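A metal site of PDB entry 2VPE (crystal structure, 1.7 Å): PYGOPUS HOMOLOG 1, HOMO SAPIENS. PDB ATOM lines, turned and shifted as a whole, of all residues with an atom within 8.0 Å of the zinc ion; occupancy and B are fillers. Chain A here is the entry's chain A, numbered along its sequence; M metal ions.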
ATOM      1  N   TYR A   6     -23.178 -14.210  17.289  1.00  0.00           N
ATOM      2  CA  TYR A   6     -22.289 -15.009  16.492  1.00  0.00           C
ATOM      3  C   TYR A   6     -20.903 -14.968  17.144  1.00  0.00           C
ATOM      4  O   TYR A   6     -20.005 -14.307  16.638  1.00  0.00           O
ATOM      5  CB  TYR A   6     -22.212 -14.424  15.084  1.00  0.00           C
ATOM      6  CG  TYR A   6     -23.440 -14.650  14.230  1.00  0.00           C
ATOM      7  CD1 TYR A   6     -23.798 -15.933  13.810  1.00  0.00           C
ATOM      8  CD2 TYR A   6     -24.220 -13.570  13.829  1.00  0.00           C
ATOM      9  CE1 TYR A   6     -24.935 -16.137  12.989  1.00  0.00           C
ATOM     10  CE2 TYR A   6     -25.337 -13.765  13.010  1.00  0.00           C
ATOM     11  CZ  TYR A   6     -25.674 -15.040  12.591  1.00  0.00           C
ATOM     12  OH  TYR A   6     -26.783 -15.230  11.769  1.00  0.00           O
ATOM     13  N   PRO A   7     -20.724 -15.697  18.250  1.00  0.00           N
ATOM     14  CA  PRO A   7     -19.396 -15.726  18.894  1.00  0.00           C
ATOM     15  C   PRO A   7     -18.353 -16.344  17.966  1.00  0.00           C
ATOM     16  O   PRO A   7     -18.612 -17.387  17.356  1.00  0.00           O
ATOM     17  CB  PRO A   7     -19.590 -16.607  20.121  1.00  0.00           C
ATOM     18  CG  PRO A   7     -21.014 -17.174  20.050  1.00  0.00           C
ATOM     19  CD  PRO A   7     -21.733 -16.581  18.885  1.00  0.00           C
ATOM     20  N   CYS A   8     -17.204 -15.676  17.838  1.00  0.00           N
ATOM     21  CA  CYS A   8     -16.116 -16.199  17.018  1.00  0.00           C
ATOM     22  C   CYS A   8     -15.729 -17.600  17.431  1.00  0.00           C
ATOM     23  O   CYS A   8     -15.524 -17.877  18.612  1.00  0.00           O
ATOM     24  CB  CYS A   8     -14.886 -15.272  17.107  1.00  0.00           C
ATOM     25  SG  CYS A   8     -13.464 -15.893  16.180  1.00  0.00           S
ATOM     26  N   GLY A   9     -15.636 -18.491  16.445  1.00  0.00           N
ATOM     27  CA  GLY A   9     -15.265 -19.891  16.674  1.00  0.00           C
ATOM     28  C   GLY A   9     -13.908 -20.025  17.392  1.00  0.00           C
ATOM     29  O   GLY A   9     -13.648 -21.040  18.046  1.00  0.00           O
ATOM     30  N   ILE A  10     -13.057 -19.008  17.262  1.00  0.00           N
ATOM     31  CA  ILE A  10     -11.740 -19.035  17.914  1.00  0.00           C
ATOM     32  C   ILE A  10     -11.696 -18.222  19.206  1.00  0.00           C
ATOM     33  O   ILE A  10     -11.395 -18.783  20.268  1.00  0.00           O
ATOM     34  CB  ILE A  10     -10.608 -18.615  16.933  1.00  0.00           C
ATOM     35  CG1 ILE A  10     -10.345 -19.740  15.930  1.00  0.00           C
ATOM     36  CG2 ILE A  10      -9.294 -18.288  17.700  1.00  0.00           C
ATOM     37  CD1 ILE A  10      -9.651 -19.286  14.652  1.00  0.00           C
ATOM     38  N   CYS A  11     -12.004 -16.922  19.139  1.00  0.00           N
ATOM     39  CA  CYS A  11     -11.785 -16.052  20.298  1.00  0.00           C
ATOM     40  C   CYS A  11     -13.019 -15.892  21.181  1.00  0.00           C
ATOM     41  O   CYS A  11     -12.899 -15.412  22.316  1.00  0.00           O
ATOM     42  CB  CYS A  11     -11.247 -14.683  19.871  1.00  0.00           C
ATOM     43  SG  CYS A  11     -12.507 -13.647  19.104  1.00  0.00           S
ATOM     44  N   THR A  12     -14.181 -16.326  20.676  1.00  0.00           N
ATOM     45  CA  THR A  12     -15.503 -16.225  21.379  1.00  0.00           C
ATOM     46  C   THR A  12     -16.127 -14.830  21.457  1.00  0.00           C
ATOM     47  O   THR A  12     -17.259 -14.689  21.916  1.00  0.00           O
ATOM     48  CB  THR A  12     -15.559 -16.921  22.803  1.00  0.00           C
ATOM     49  OG1 THR A  12     -14.921 -16.087  23.793  1.00  0.00           O
ATOM     50  CG2 THR A  12     -14.961 -18.300  22.783  1.00  0.00           C
ATOM     51  N   ASN A  13     -15.402 -13.802  20.995  1.00  0.00           N
ATOM     52  CA  ASN A  13     -15.969 -12.463  20.935  1.00  0.00           C
ATOM     53  C   ASN A  13     -16.927 -12.383  19.764  1.00  0.00           C
ATOM     54  O   ASN A  13     -16.757 -13.096  18.767  1.00  0.00           O
ATOM     55  CB  ASN A  13     -14.861 -11.434  20.730  1.00  0.00           C
ATOM     56  CG  ASN A  13     -13.879 -11.415  21.878  1.00  0.00           C
ATOM     57  OD1 ASN A  13     -12.668 -11.424  21.662  1.00  0.00           O
ATOM     58  ND2 ASN A  13     -14.391 -11.407  23.098  1.00  0.00           N
ATOM     59  N   GLU A  14     -17.901 -11.486  19.873  1.00  0.00           N
ATOM     60  CA  GLU A  14     -18.893 -11.276  18.834  1.00  0.00           C
ATOM     61  C   GLU A  14     -18.239 -11.017  17.477  1.00  0.00           C
ATOM     62  O   GLU A  14     -17.254 -10.272  17.366  1.00  0.00           O
ATOM     63  CB  GLU A  14     -19.810 -10.103  19.219  1.00  0.00           C
ATOM     64  CG  GLU A  14     -20.895  -9.778  18.211  1.00  0.00           C
ATOM     65  CD  GLU A  14     -21.997 -10.835  18.148  1.00  0.00           C
ATOM     66  OE1 GLU A  14     -23.142 -10.538  18.562  1.00  0.00           O
ATOM     67  OE2 GLU A  14     -21.715 -11.959  17.695  1.00  0.00           O
ATOM     68  N   VAL A  15     -18.796 -11.642  16.446  1.00  0.00           N
ATOM     69  CA  VAL A  15     -18.408 -11.363  15.081  1.00  0.00           C
ATOM     70  C   VAL A  15     -19.399 -10.331  14.533  1.00  0.00           C
ATOM     71  O   VAL A  15     -20.572 -10.671  14.245  1.00  0.00           O
ATOM     72  CB  VAL A  15     -18.382 -12.631  14.226  1.00  0.00           C
ATOM     73  CG1 VAL A  15     -18.087 -12.284  12.757  1.00  0.00           C
ATOM     74  CG2 VAL A  15     -17.315 -13.594  14.757  1.00  0.00           C
ATOM     75  N   GLN A  19     -16.604  -6.254  10.680  1.00  0.00           N
ATOM     76  CA  GLN A  19     -15.314  -6.931  10.846  1.00  0.00           C
ATOM     77  C   GLN A  19     -15.111  -7.938   9.719  1.00  0.00           C
ATOM     78  O   GLN A  19     -16.079  -8.567   9.255  1.00  0.00           O
ATOM     79  CB  GLN A  19     -15.235  -7.660  12.198  1.00  0.00           C
ATOM     80  CG  GLN A  19     -15.287  -6.786  13.458  1.00  0.00           C
ATOM     81  CD  GLN A  19     -15.445  -7.602  14.753  1.00  0.00           C
ATOM     82  OE1 GLN A  19     -16.173  -8.598  14.811  1.00  0.00           O
ATOM     83  NE2 GLN A  19     -14.780  -7.159  15.798  1.00  0.00           N
ATOM     84  N   ASP A  20     -13.861  -8.129   9.269  1.00  0.00           N
ATOM     85  CA  ASP A  20     -13.558  -9.220   8.324  1.00  0.00           C
ATOM     86  C   ASP A  20     -13.807 -10.521   9.075  1.00  0.00           C
ATOM     87  O   ASP A  20     -13.208 -10.756  10.126  1.00  0.00           O
ATOM     88  CB  ASP A  20     -12.102  -9.228   7.867  1.00  0.00           C
ATOM     89  CG  ASP A  20     -11.734  -8.058   6.942  1.00  0.00           C
ATOM     90  OD1 ASP A  20     -12.614  -7.272   6.520  1.00  0.00           O
ATOM     91  OD2 ASP A  20     -10.530  -7.937   6.622  1.00  0.00           O
ATOM     92  N   ALA A  21     -14.663 -11.362   8.526  1.00  0.00           N
ATOM     93  CA  ALA A  21     -15.001 -12.619   9.175  1.00  0.00           C
ATOM     94  C   ALA A  21     -15.605 -13.541   8.150  1.00  0.00           C
ATOM     95  O   ALA A  21     -16.183 -13.075   7.164  1.00  0.00           O
ATOM     96  CB  ALA A  21     -15.970 -12.392  10.324  1.00  0.00           C
ATOM     97  N   TRP A  31     -19.097 -18.483  12.762  1.00  0.00           N
ATOM     98  CA  TRP A  31     -18.358 -17.373  12.169  1.00  0.00           C
ATOM     99  C   TRP A  31     -16.987 -17.240  12.844  1.00  0.00           C
ATOM    100  O   TRP A  31     -16.852 -17.529  14.055  1.00  0.00           O
ATOM    101  CB  TRP A  31     -19.144 -16.091  12.317  1.00  0.00           C
ATOM    102  CG  TRP A  31     -20.215 -15.962  11.293  1.00  0.00           C
ATOM    103  CD1 TRP A  31     -21.504 -16.393  11.395  1.00  0.00           C
ATOM    104  CD2 TRP A  31     -20.074 -15.400   9.997  1.00  0.00           C
ATOM    105  NE1 TRP A  31     -22.187 -16.101  10.243  1.00  0.00           N
ATOM    106  CE2 TRP A  31     -21.334 -15.502   9.356  1.00  0.00           C
ATOM    107  CE3 TRP A  31     -19.006 -14.802   9.303  1.00  0.00           C
ATOM    108  CZ2 TRP A  31     -21.559 -15.037   8.047  1.00  0.00           C
ATOM    109  CZ3 TRP A  31     -19.225 -14.317   8.007  1.00  0.00           C
ATOM    110  CH2 TRP A  31     -20.491 -14.457   7.384  1.00  0.00           C
ATOM    111  N   PHE A  32     -15.990 -16.820  12.059  1.00  0.00           N
ATOM    112  CA  PHE A  32     -14.639 -16.660  12.585  1.00  0.00           C
ATOM    113  C   PHE A  32     -14.106 -15.328  12.088  1.00  0.00           C
ATOM    114  O   PHE A  32     -14.156 -15.058  10.891  1.00  0.00           O
ATOM    115  CB  PHE A  32     -13.724 -17.749  12.030  1.00  0.00           C
ATOM    116  CG  PHE A  32     -14.022 -19.140  12.555  1.00  0.00           C
ATOM    117  CD1 PHE A  32     -13.165 -19.723  13.488  1.00  0.00           C
ATOM    118  CD2 PHE A  32     -15.112 -19.852  12.095  1.00  0.00           C
ATOM    119  CE1 PHE A  32     -13.422 -21.020  13.989  1.00  0.00           C
ATOM    120  CE2 PHE A  32     -15.360 -21.158  12.575  1.00  0.00           C
ATOM    121  CZ  PHE A  32     -14.524 -21.733  13.500  1.00  0.00           C
ATOM    122  N   HIS A  33     -13.567 -14.506  12.980  1.00  0.00           N
ATOM    123  CA  HIS A  33     -12.825 -13.302  12.546  1.00  0.00           C
ATOM    124  C   HIS A  33     -11.683 -13.749  11.615  1.00  0.00           C
ATOM    125  O   HIS A  33     -10.984 -14.721  11.916  1.00  0.00           O
ATOM    126  CB  HIS A  33     -12.207 -12.585  13.748  1.00  0.00           C
ATOM    127  CG  HIS A  33     -13.207 -12.027  14.705  1.00  0.00           C
ATOM    128  ND1 HIS A  33     -13.304 -12.463  16.010  1.00  0.00           N
ATOM    129  CD2 HIS A  33     -14.136 -11.053  14.565  1.00  0.00           C
ATOM    130  CE1 HIS A  33     -14.260 -11.790  16.630  1.00  0.00           C
ATOM    131  NE2 HIS A  33     -14.779 -10.923  15.770  1.00  0.00           N
ATOM    132  N   ARG A  34     -11.503 -13.031  10.510  1.00  0.00           N
ATOM    133  CA  ARG A  34     -10.394 -13.305   9.576  1.00  0.00           C
ATOM    134  C   ARG A  34      -9.053 -13.350  10.342  1.00  0.00           C
ATOM    135  O   ARG A  34      -8.232 -14.276  10.163  1.00  0.00           O
ATOM    136  CB  ARG A  34     -10.335 -12.207   8.510  1.00  0.00           C
ATOM    137  CG  ARG A  34      -9.195 -12.404   7.530  1.00  0.00           C
ATOM    138  CD  ARG A  34      -9.043 -11.231   6.560  1.00  0.00           C
ATOM    139  NE  ARG A  34      -8.725  -9.952   7.236  1.00  0.00           N
ATOM    140  CZ  ARG A  34      -7.524  -9.649   7.740  1.00  0.00           C
ATOM    141  NH1 ARG A  34      -6.542 -10.535   7.726  1.00  0.00           N
ATOM    142  NH2 ARG A  34      -7.328  -8.456   8.298  1.00  0.00           N
ATOM    143  N   ILE A  35      -8.838 -12.345  11.176  1.00  0.00           N
ATOM    144  CA  ILE A  35      -7.568 -12.247  11.919  1.00  0.00           C
ATOM    145  C   ILE A  35      -7.337 -13.489  12.795  1.00  0.00           C
ATOM    146  O   ILE A  35      -6.254 -14.079  12.776  1.00  0.00           O
ATOM    147  CB  ILE A  35      -7.538 -10.955  12.734  1.00  0.00           C
ATOM    148  CG1 ILE A  35      -7.414  -9.758  11.764  1.00  0.00           C
ATOM    149  CG2 ILE A  35      -6.370 -11.005  13.719  1.00  0.00           C
ATOM    150  CD1 ILE A  35      -7.459  -8.403  12.389  1.00  0.00           C
ATOM    151  N   CYS A  36      -8.375 -13.906  13.522  1.00  0.00           N
ATOM    152  CA  CYS A  36      -8.271 -15.093  14.373  1.00  0.00           C
ATOM    153  C   CYS A  36      -7.806 -16.339  13.609  1.00  0.00           C
ATOM    154  O   CYS A  36      -7.020 -17.135  14.124  1.00  0.00           O
ATOM    155  CB  CYS A  36      -9.602 -15.340  15.091  1.00  0.00           C
ATOM    156  SG  CYS A  36      -9.907 -14.065  16.298  1.00  0.00           S
ATOM    157  N   THR A  37      -8.271 -16.467  12.368  1.00  0.00           N
ATOM    158  CA  THR A  37      -7.963 -17.656  11.575  1.00  0.00           C
ATOM    159  C   THR A  37      -6.540 -17.636  11.001  1.00  0.00           C
ATOM    160  O   THR A  37      -6.043 -18.665  10.596  1.00  0.00           O
ATOM    161  CB  THR A  37      -8.948 -17.865  10.410  1.00  0.00           C
ATOM    162  OG1 THR A  37      -8.749 -16.839   9.430  1.00  0.00           O
ATOM    163  CG2 THR A  37     -10.418 -17.884  10.880  1.00  0.00           C
HETATM  164 ZN    ZN M   1     -12.183 -14.058  16.778  1.00  0.00          ZN
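The backbone carbonyl oxygen (O) of Glu 14 lies within hydrogen-bond range of a ring nitrogen (NE2) of His 33 (3.0 Å).
The backbone NH (N) of Cys 8 is in hydrogen-bond range of the backbone carbonyl oxygen (O) of Asn 13, at 2.8 Å.
NE2 of His 33 is in hydrogen-bond range of OE1 of Gln 19.
The backbone NH of Ile 10 lies close to the side-chain sulfur of Cys 8 (3.3 Å).
The side-chain sulfur (SG) of Cys 11 sits close to the side-chain amide oxygen (OD1) of Asn 13.
Of the 20 residues printed, 4 come within 4 Å of the zinc ion.
The zinc ion is bound by a ring nitrogen (ND1) of His 33 (2.1 Å), the side-chain sulfur of Cys 8 (2.3 Å), the side-chain sulfur of Cys 36 (2.3 Å) and the side-chain sulfur of Cys 11 (2.4 Å).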
